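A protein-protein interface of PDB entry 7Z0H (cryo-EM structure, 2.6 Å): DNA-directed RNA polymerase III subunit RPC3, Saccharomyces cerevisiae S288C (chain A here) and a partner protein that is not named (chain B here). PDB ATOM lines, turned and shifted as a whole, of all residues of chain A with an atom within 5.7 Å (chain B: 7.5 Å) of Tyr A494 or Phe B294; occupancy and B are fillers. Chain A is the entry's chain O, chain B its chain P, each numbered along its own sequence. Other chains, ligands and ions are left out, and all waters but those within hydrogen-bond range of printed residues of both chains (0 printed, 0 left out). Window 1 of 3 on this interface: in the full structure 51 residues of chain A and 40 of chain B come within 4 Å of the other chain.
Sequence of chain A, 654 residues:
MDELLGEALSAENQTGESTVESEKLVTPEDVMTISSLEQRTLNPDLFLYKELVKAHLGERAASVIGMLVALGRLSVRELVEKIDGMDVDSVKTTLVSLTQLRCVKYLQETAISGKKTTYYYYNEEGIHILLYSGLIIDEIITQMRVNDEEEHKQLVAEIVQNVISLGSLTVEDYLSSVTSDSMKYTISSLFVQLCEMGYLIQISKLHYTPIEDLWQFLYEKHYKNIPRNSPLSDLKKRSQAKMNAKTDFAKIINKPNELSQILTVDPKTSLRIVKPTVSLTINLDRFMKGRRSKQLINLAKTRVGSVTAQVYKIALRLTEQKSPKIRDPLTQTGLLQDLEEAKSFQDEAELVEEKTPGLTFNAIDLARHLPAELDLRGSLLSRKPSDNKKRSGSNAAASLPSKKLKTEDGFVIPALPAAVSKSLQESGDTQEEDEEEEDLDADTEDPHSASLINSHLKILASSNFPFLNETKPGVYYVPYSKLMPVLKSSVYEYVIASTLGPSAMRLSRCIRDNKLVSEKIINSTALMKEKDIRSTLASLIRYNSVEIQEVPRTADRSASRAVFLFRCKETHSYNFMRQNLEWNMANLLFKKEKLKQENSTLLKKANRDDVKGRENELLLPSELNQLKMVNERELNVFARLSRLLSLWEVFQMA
The side-chain hydroxyl of Thr A302 lies close to the side-chain amide oxygen of Asn B295 (3.4 Å).
The side-chain hydroxyl (OH) of Tyr A494 lies within hydrogen-bond range of the backbone carbonyl oxygen (O) of Phe B294 (2.8 Å).
The backbone carbonyl oxygen (O) of Val A495 is in hydrogen-bond range of the side-chain hydroxyl (OG1) of Thr A499 (2.6 Å).
The side-chain hydroxyl of Ser B292 is in hydrogen-bond range of the side-chain amide oxygen of Asn B295 (2.8 Å).
CD1 of Leu A299 touches CE2 of Phe B294 (3.7 Å).
Thr A302 touches Ile B268.
Ser B292 touches Thr A302.
CB of Phe B294 touches CG2 of Thr A302 (3.6 Å).
Ile B293 touches Val A491.
CE2 of Tyr A494 touches O of Ile B293, at 2.9 Å.
Tyr A494 touches Tyr B296 (CE2 to CD1, 3.4 Å).
OH of Tyr B296 touches O of Ala A497, at 3.8 Å.
CZ of Tyr B296 touches CA of Ser A498, at 3.97 Å.
CD2 of Phe B312 touches OG1 of Thr A499, at 3.0 Å.
Tyr A494 touches just these residues of chain B: Ile B293 (2.9 Å), Phe B294 (2.8 Å) and Tyr B296 (3.4 Å).
Of chain A, only Leu A299 (3.7 Å), Thr A302 (3.6 Å) and Tyr A494 (2.8 Å) come within 4 Å of Phe B294.
Of the printed residues of chain A, Ile B268 touches Thr A302 (3.1 Å).
Of the printed residues of chain B, Ser A498 touches Tyr B296.
Of the printed residues of chain B, Ala A497 touches Tyr B296 (3.8 Å).
Printed residues of chain B within 4 Å of Thr A499: Phe B312 (3.0 Å).
The nearest residue of chain B that does not touch Tyr A494 is Asp B251 (4.1 Å).
The nearest residue of chain A that does not touch Phe B294 is Ser A490 (4.1 Å).
The nearest printed residue of chain A that does not touch Ile B293 is Val A495 (4.2 Å).
Of the 12 printed residues of chain B, 8 touch a printed residue of chain A.
Hydrophobic or aromatic side chains of chain B that line the printed part of chain A: Leu B265, Ile B268, Ile B293, Phe B294, Tyr B296 and Phe B312.
Hydrophobic or aromatic side chains of chain A within 4 Å of the printed part of chain B: Leu A299, Val A491 and Tyr A494.
Along chain A the printed residues that touch a printed residue of chain B span positions 299 to 499.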
ATOM      1  N   LEU A 299      -6.051   7.436  -7.432  1.00  0.00           N
ATOM      2  CA  LEU A 299      -6.360   8.043  -6.143  1.00  0.00           C
ATOM      3  C   LEU A 299      -5.917   9.499  -6.114  1.00  0.00           C
ATOM      4  O   LEU A 299      -6.672  10.385  -5.701  1.00  0.00           O
ATOM      5  CB  LEU A 299      -5.683   7.241  -5.024  1.00  0.00           C
ATOM      6  CG  LEU A 299      -5.726   7.722  -3.570  1.00  0.00           C
ATOM      7  CD1 LEU A 299      -5.726   6.530  -2.630  1.00  0.00           C
ATOM      8  CD2 LEU A 299      -4.547   8.632  -3.248  1.00  0.00           C
ATOM      9  N   THR A 302      -8.102  11.682  -8.206  1.00  0.00           N
ATOM     10  CA  THR A 302      -9.304  12.029  -7.459  1.00  0.00           C
ATOM     11  C   THR A 302      -8.984  12.930  -6.273  1.00  0.00           C
ATOM     12  O   THR A 302      -9.790  13.792  -5.910  1.00  0.00           O
ATOM     13  CB  THR A 302     -10.016  10.764  -6.981  1.00  0.00           C
ATOM     14  OG1 THR A 302     -10.092   9.817  -8.056  1.00  0.00           O
ATOM     15  CG2 THR A 302     -11.419  11.097  -6.504  1.00  0.00           C
ATOM     16  N   LEU A 487      -4.426   2.652   3.545  1.00  0.00           N
ATOM     17  CA  LEU A 487      -4.979   2.519   2.201  1.00  0.00           C
ATOM     18  C   LEU A 487      -6.115   1.506   2.179  1.00  0.00           C
ATOM     19  O   LEU A 487      -7.154   1.736   1.543  1.00  0.00           O
ATOM     20  CB  LEU A 487      -3.880   2.119   1.217  1.00  0.00           C
ATOM     21  CG  LEU A 487      -4.323   1.732  -0.196  1.00  0.00           C
ATOM     22  CD1 LEU A 487      -5.112   2.860  -0.845  1.00  0.00           C
ATOM     23  CD2 LEU A 487      -3.128   1.347  -1.053  1.00  0.00           C
ATOM     24  N   SER A 489      -8.021   0.712   4.740  1.00  0.00           N
ATOM     25  CA  SER A 489      -9.137   1.346   5.432  1.00  0.00           C
ATOM     26  C   SER A 489      -9.870   2.310   4.510  1.00  0.00           C
ATOM     27  O   SER A 489     -11.103   2.296   4.438  1.00  0.00           O
ATOM     28  CB  SER A 489      -8.635   2.069   6.682  1.00  0.00           C
ATOM     29  OG  SER A 489      -9.716   2.473   7.506  1.00  0.00           O
ATOM     30  N   SER A 490      -9.125   3.141   3.779  1.00  0.00           N
ATOM     31  CA  SER A 490      -9.752   4.121   2.899  1.00  0.00           C
ATOM     32  C   SER A 490     -10.560   3.442   1.799  1.00  0.00           C
ATOM     33  O   SER A 490     -11.711   3.817   1.539  1.00  0.00           O
ATOM     34  CB  SER A 490      -8.687   5.039   2.298  1.00  0.00           C
ATOM     35  OG  SER A 490      -7.759   4.306   1.519  1.00  0.00           O
ATOM     36  N   VAL A 491      -9.978   2.429   1.149  1.00  0.00           N
ATOM     37  CA  VAL A 491     -10.668   1.801   0.025  1.00  0.00           C
ATOM     38  C   VAL A 491     -11.901   1.042   0.505  1.00  0.00           C
ATOM     39  O   VAL A 491     -12.984   1.161  -0.086  1.00  0.00           O
ATOM     40  CB  VAL A 491      -9.702   0.907  -0.780  1.00  0.00           C
ATOM     41  CG1 VAL A 491      -9.160  -0.243   0.057  1.00  0.00           C
ATOM     42  CG2 VAL A 491     -10.388   0.379  -2.030  1.00  0.00           C
ATOM     43  N   TYR A 492     -11.777   0.278   1.598  1.00  0.00           N
ATOM     44  CA  TYR A 492     -12.937  -0.431   2.128  1.00  0.00           C
ATOM     45  C   TYR A 492     -14.016   0.541   2.582  1.00  0.00           C
ATOM     46  O   TYR A 492     -15.210   0.315   2.342  1.00  0.00           O
ATOM     47  CB  TYR A 492     -12.522  -1.336   3.287  1.00  0.00           C
ATOM     48  CG  TYR A 492     -13.699  -1.902   4.048  1.00  0.00           C
ATOM     49  CD1 TYR A 492     -14.431  -2.967   3.542  1.00  0.00           C
ATOM     50  CD2 TYR A 492     -14.089  -1.360   5.267  1.00  0.00           C
ATOM     51  CE1 TYR A 492     -15.509  -3.484   4.230  1.00  0.00           C
ATOM     52  CE2 TYR A 492     -15.169  -1.869   5.962  1.00  0.00           C
ATOM     53  CZ  TYR A 492     -15.876  -2.930   5.438  1.00  0.00           C
ATOM     54  OH  TYR A 492     -16.950  -3.443   6.127  1.00  0.00           O
ATOM     55  N   GLU A 493     -13.615   1.632   3.238  1.00  0.00           N
ATOM     56  CA  GLU A 493     -14.589   2.574   3.767  1.00  0.00           C
ATOM     57  C   GLU A 493     -15.333   3.277   2.646  1.00  0.00           C
ATOM     58  O   GLU A 493     -16.549   3.482   2.733  1.00  0.00           O
ATOM     59  CB  GLU A 493     -13.892   3.588   4.670  1.00  0.00           C
ATOM     60  CG  GLU A 493     -14.848   4.513   5.378  1.00  0.00           C
ATOM     61  CD  GLU A 493     -15.271   3.953   6.718  1.00  0.00           C
ATOM     62  OE1 GLU A 493     -14.882   2.809   7.032  1.00  0.00           O
ATOM     63  OE2 GLU A 493     -15.996   4.647   7.453  1.00  0.00           O
ATOM     64  N   TYR A 494     -14.632   3.646   1.574  1.00  0.00           N
ATOM     65  CA  TYR A 494     -15.342   4.301   0.485  1.00  0.00           C
ATOM     66  C   TYR A 494     -16.168   3.309  -0.326  1.00  0.00           C
ATOM     67  O   TYR A 494     -17.171   3.701  -0.929  1.00  0.00           O
ATOM     68  CB  TYR A 494     -14.382   5.060  -0.425  1.00  0.00           C
ATOM     69  CG  TYR A 494     -15.060   6.249  -1.065  1.00  0.00           C
ATOM     70  CD1 TYR A 494     -15.088   7.482  -0.425  1.00  0.00           C
ATOM     71  CD2 TYR A 494     -15.730   6.124  -2.271  1.00  0.00           C
ATOM     72  CE1 TYR A 494     -15.725   8.568  -0.992  1.00  0.00           C
ATOM     73  CE2 TYR A 494     -16.375   7.204  -2.841  1.00  0.00           C
ATOM     74  CZ  TYR A 494     -16.370   8.422  -2.200  1.00  0.00           C
ATOM     75  OH  TYR A 494     -17.010   9.495  -2.775  1.00  0.00           O
ATOM     76  N   VAL A 495     -15.788   2.027  -0.341  1.00  0.00           N
ATOM     77  CA  VAL A 495     -16.669   1.014  -0.920  1.00  0.00           C
ATOM     78  C   VAL A 495     -17.966   0.930  -0.122  1.00  0.00           C
ATOM     79  O   VAL A 495     -19.068   0.913  -0.686  1.00  0.00           O
ATOM     80  CB  VAL A 495     -15.953  -0.347  -0.988  1.00  0.00           C
ATOM     81  CG1 VAL A 495     -16.966  -1.476  -1.091  1.00  0.00           C
ATOM     82  CG2 VAL A 495     -14.990  -0.384  -2.166  1.00  0.00           C
ATOM     83  N   ILE A 496     -17.852   0.896   1.207  1.00  0.00           N
ATOM     84  CA  ILE A 496     -19.042   0.888   2.058  1.00  0.00           C
ATOM     85  C   ILE A 496     -19.860   2.153   1.837  1.00  0.00           C
ATOM     86  O   ILE A 496     -21.098   2.131   1.875  1.00  0.00           O
ATOM     87  CB  ILE A 496     -18.644   0.722   3.537  1.00  0.00           C
ATOM     88  CG1 ILE A 496     -17.883  -0.587   3.747  1.00  0.00           C
ATOM     89  CG2 ILE A 496     -19.873   0.773   4.436  1.00  0.00           C
ATOM     90  CD1 ILE A 496     -18.761  -1.821   3.715  1.00  0.00           C
ATOM     91  N   ALA A 497     -19.180   3.281   1.620  1.00  0.00           N
ATOM     92  CA  ALA A 497     -19.878   4.534   1.360  1.00  0.00           C
ATOM     93  C   ALA A 497     -20.654   4.479   0.050  1.00  0.00           C
ATOM     94  O   ALA A 497     -21.817   4.892  -0.013  1.00  0.00           O
ATOM     95  CB  ALA A 497     -18.883   5.694   1.351  1.00  0.00           C
ATOM     96  N   SER A 498     -20.029   3.965  -1.009  1.00  0.00           N
ATOM     97  CA  SER A 498     -20.741   3.803  -2.271  1.00  0.00           C
ATOM     98  C   SER A 498     -21.868   2.786  -2.144  1.00  0.00           C
ATOM     99  O   SER A 498     -22.812   2.803  -2.942  1.00  0.00           O
ATOM    100  CB  SER A 498     -19.766   3.389  -3.372  1.00  0.00           C
ATOM    101  OG  SER A 498     -20.444   3.191  -4.599  1.00  0.00           O
ATOM    102  N   THR A 499     -21.788   1.900  -1.150  1.00  0.00           N
ATOM    103  CA  THR A 499     -22.826   0.887  -0.983  1.00  0.00           C
ATOM    104  C   THR A 499     -24.028   1.433  -0.215  1.00  0.00           C
ATOM    105  O   THR A 499     -25.177   1.115  -0.547  1.00  0.00           O
ATOM    106  CB  THR A 499     -22.248  -0.335  -0.269  1.00  0.00           C
ATOM    107  OG1 THR A 499     -21.035  -0.734  -0.916  1.00  0.00           O
ATOM    108  CG2 THR A 499     -23.233  -1.495  -0.323  1.00  0.00           C
ATOM    109  N   ASP B 251     -16.107  12.291   5.531  1.00  0.00           N
ATOM    110  CA  ASP B 251     -14.997  12.757   4.656  1.00  0.00           C
ATOM    111  C   ASP B 251     -14.928  14.282   4.712  1.00  0.00           C
ATOM    112  O   ASP B 251     -14.913  14.910   3.634  1.00  0.00           O
ATOM    113  CB  ASP B 251     -15.169  12.272   3.214  1.00  0.00           C
ATOM    114  CG  ASP B 251     -13.857  11.905   2.542  1.00  0.00           C
ATOM    115  OD1 ASP B 251     -12.799  12.325   3.054  1.00  0.00           O
ATOM    116  OD2 ASP B 251     -13.902  11.198   1.517  1.00  0.00           O
ATOM    117  N   LEU B 265     -10.748  16.568  -2.213  1.00  0.00           N
ATOM    118  CA  LEU B 265     -11.641  16.279  -3.333  1.00  0.00           C
ATOM    119  C   LEU B 265     -13.052  16.811  -3.099  1.00  0.00           C
ATOM    120  O   LEU B 265     -14.019  16.284  -3.667  1.00  0.00           O
ATOM    121  CB  LEU B 265     -11.682  14.776  -3.624  1.00  0.00           C
ATOM    122  CG  LEU B 265     -12.169  13.771  -2.574  1.00  0.00           C
ATOM    123  CD1 LEU B 265     -12.745  12.547  -3.265  1.00  0.00           C
ATOM    124  CD2 LEU B 265     -11.053  13.356  -1.629  1.00  0.00           C
ATOM    125  N   ILE B 268     -14.725  18.170  -6.261  1.00  0.00           N
ATOM    126  CA  ILE B 268     -15.088  17.060  -7.135  1.00  0.00           C
ATOM    127  C   ILE B 268     -16.350  16.373  -6.632  1.00  0.00           C
ATOM    128  O   ILE B 268     -17.221  15.987  -7.423  1.00  0.00           O
ATOM    129  CB  ILE B 268     -13.909  16.080  -7.259  1.00  0.00           C
ATOM    130  CG1 ILE B 268     -12.630  16.854  -7.588  1.00  0.00           C
ATOM    131  CG2 ILE B 268     -14.192  15.031  -8.321  1.00  0.00           C
ATOM    132  CD1 ILE B 268     -11.368  16.167  -7.155  1.00  0.00           C
ATOM    133  N   LEU B 269     -16.473  16.203  -5.313  1.00  0.00           N
ATOM    134  CA  LEU B 269     -17.691  15.612  -4.763  1.00  0.00           C
ATOM    135  C   LEU B 269     -18.898  16.516  -4.995  1.00  0.00           C
ATOM    136  O   LEU B 269     -19.945  16.065  -5.473  1.00  0.00           O
ATOM    137  CB  LEU B 269     -17.513  15.324  -3.271  1.00  0.00           C
ATOM    138  CG  LEU B 269     -18.587  14.453  -2.609  1.00  0.00           C
ATOM    139  CD1 LEU B 269     -17.966  13.489  -1.610  1.00  0.00           C
ATOM    140  CD2 LEU B 269     -19.661  15.297  -1.935  1.00  0.00           C
ATOM    141  N   PHE B 291     -11.129   2.775 -11.790  1.00  0.00           N
ATOM    142  CA  PHE B 291     -12.503   3.257 -11.727  1.00  0.00           C
ATOM    143  C   PHE B 291     -12.578   4.608 -11.020  1.00  0.00           C
ATOM    144  O   PHE B 291     -13.550   5.348 -11.184  1.00  0.00           O
ATOM    145  CB  PHE B 291     -13.398   2.231 -11.020  1.00  0.00           C
ATOM    146  CG  PHE B 291     -14.731   2.782 -10.585  1.00  0.00           C
ATOM    147  CD1 PHE B 291     -15.679   3.161 -11.519  1.00  0.00           C
ATOM    148  CD2 PHE B 291     -15.030   2.922  -9.242  1.00  0.00           C
ATOM    149  CE1 PHE B 291     -16.900   3.670 -11.120  1.00  0.00           C
ATOM    150  CE2 PHE B 291     -16.249   3.431  -8.836  1.00  0.00           C
ATOM    151  CZ  PHE B 291     -17.185   3.805  -9.776  1.00  0.00           C
ATOM    152  N   SER B 292     -11.533   4.933 -10.257  1.00  0.00           N
ATOM    153  CA  SER B 292     -11.514   6.119  -9.401  1.00  0.00           C
ATOM    154  C   SER B 292     -12.671   6.065  -8.403  1.00  0.00           C
ATOM    155  O   SER B 292     -13.600   6.874  -8.433  1.00  0.00           O
ATOM    156  CB  SER B 292     -11.550   7.409 -10.229  1.00  0.00           C
ATOM    157  OG  SER B 292     -12.879   7.757 -10.575  1.00  0.00           O
ATOM    158  N   ILE B 293     -12.598   5.067  -7.516  1.00  0.00           N
ATOM    159  CA  ILE B 293     -13.714   4.764  -6.626  1.00  0.00           C
ATOM    160  C   ILE B 293     -14.043   5.947  -5.728  1.00  0.00           C
ATOM    161  O   ILE B 293     -15.194   6.111  -5.308  1.00  0.00           O
ATOM    162  CB  ILE B 293     -13.412   3.498  -5.797  1.00  0.00           C
ATOM    163  CG1 ILE B 293     -12.569   3.839  -4.567  1.00  0.00           C
ATOM    164  CG2 ILE B 293     -12.695   2.461  -6.647  1.00  0.00           C
ATOM    165  CD1 ILE B 293     -12.651   2.810  -3.466  1.00  0.00           C
ATOM    166  N   PHE B 294     -13.058   6.802  -5.439  1.00  0.00           N
ATOM    167  CA  PHE B 294     -13.260   7.873  -4.469  1.00  0.00           C
ATOM    168  C   PHE B 294     -14.215   8.948  -4.972  1.00  0.00           C
ATOM    169  O   PHE B 294     -14.629   9.808  -4.189  1.00  0.00           O
ATOM    170  CB  PHE B 294     -11.914   8.486  -4.086  1.00  0.00           C
ATOM    171  CG  PHE B 294     -11.021   7.548  -3.324  1.00  0.00           C
ATOM    172  CD1 PHE B 294     -11.090   7.476  -1.943  1.00  0.00           C
ATOM    173  CD2 PHE B 294     -10.122   6.732  -3.988  1.00  0.00           C
ATOM    174  CE1 PHE B 294     -10.274   6.612  -1.238  1.00  0.00           C
ATOM    175  CE2 PHE B 294      -9.302   5.867  -3.290  1.00  0.00           C
ATOM    176  CZ  PHE B 294      -9.378   5.807  -1.912  1.00  0.00           C
ATOM    177  N   ASN B 295     -14.565   8.930  -6.257  1.00  0.00           N
ATOM    178  CA  ASN B 295     -15.631   9.770  -6.790  1.00  0.00           C
ATOM    179  C   ASN B 295     -16.461   8.939  -7.758  1.00  0.00           C
ATOM    180  O   ASN B 295     -15.956   8.490  -8.792  1.00  0.00           O
ATOM    181  CB  ASN B 295     -15.077  11.034  -7.461  1.00  0.00           C
ATOM    182  CG  ASN B 295     -14.147  10.734  -8.621  1.00  0.00           C
ATOM    183  OD1 ASN B 295     -13.461   9.713  -8.635  1.00  0.00           O
ATOM    184  ND2 ASN B 295     -14.118  11.629  -9.601  1.00  0.00           N
ATOM    185  N   TYR B 296     -17.728   8.721  -7.409  1.00  0.00           N
ATOM    186  CA  TYR B 296     -18.626   7.902  -8.208  1.00  0.00           C
ATOM    187  C   TYR B 296     -19.873   8.647  -8.655  1.00  0.00           C
ATOM    188  O   TYR B 296     -20.737   8.042  -9.297  1.00  0.00           O
ATOM    189  CB  TYR B 296     -19.039   6.645  -7.428  1.00  0.00           C
ATOM    190  CG  TYR B 296     -19.738   6.943  -6.121  1.00  0.00           C
ATOM    191  CD1 TYR B 296     -19.011   7.179  -4.962  1.00  0.00           C
ATOM    192  CD2 TYR B 296     -21.125   6.987  -6.044  1.00  0.00           C
ATOM    193  CE1 TYR B 296     -19.642   7.456  -3.765  1.00  0.00           C
ATOM    194  CE2 TYR B 296     -21.765   7.260  -4.849  1.00  0.00           C
ATOM    195  CZ  TYR B 296     -21.019   7.494  -3.713  1.00  0.00           C
ATOM    196  OH  TYR B 296     -21.648   7.767  -2.521  1.00  0.00           O
ATOM    197  N   PHE B 297     -19.999   9.933  -8.329  1.00  0.00           N
ATOM    198  CA  PHE B 297     -21.153  10.716  -8.748  1.00  0.00           C
ATOM    199  C   PHE B 297     -21.122  11.061 -10.230  1.00  0.00           C
ATOM    200  O   PHE B 297     -22.144  11.501 -10.767  1.00  0.00           O
ATOM    201  CB  PHE B 297     -21.239  11.981  -7.896  1.00  0.00           C
ATOM    202  CG  PHE B 297     -21.216  11.704  -6.421  1.00  0.00           C
ATOM    203  CD1 PHE B 297     -22.204  10.928  -5.836  1.00  0.00           C
ATOM    204  CD2 PHE B 297     -20.189  12.181  -5.626  1.00  0.00           C
ATOM    205  CE1 PHE B 297     -22.183  10.660  -4.482  1.00  0.00           C
ATOM    206  CE2 PHE B 297     -20.162  11.911  -4.274  1.00  0.00           C
ATOM    207  CZ  PHE B 297     -21.160  11.151  -3.701  1.00  0.00           C
ATOM    208  N   PHE B 312     -24.279  -5.251  -4.591  1.00  0.00           N
ATOM    209  CA  PHE B 312     -23.433  -5.625  -3.463  1.00  0.00           C
ATOM    210  C   PHE B 312     -24.185  -6.425  -2.409  1.00  0.00           C
ATOM    211  O   PHE B 312     -23.549  -7.043  -1.549  1.00  0.00           O
ATOM    212  CB  PHE B 312     -22.814  -4.380  -2.827  1.00  0.00           C
ATOM    213  CG  PHE B 312     -21.551  -3.920  -3.499  1.00  0.00           C
ATOM    214  CD1 PHE B 312     -20.905  -4.729  -4.421  1.00  0.00           C
ATOM    215  CD2 PHE B 312     -21.004  -2.684  -3.202  1.00  0.00           C
ATOM    216  CE1 PHE B 312     -19.742  -4.307  -5.039  1.00  0.00           C
ATOM    217  CE2 PHE B 312     -19.841  -2.257  -3.817  1.00  0.00           C
ATOM    218  CZ  PHE B 312     -19.209  -3.071  -4.737  1.00  0.00           C
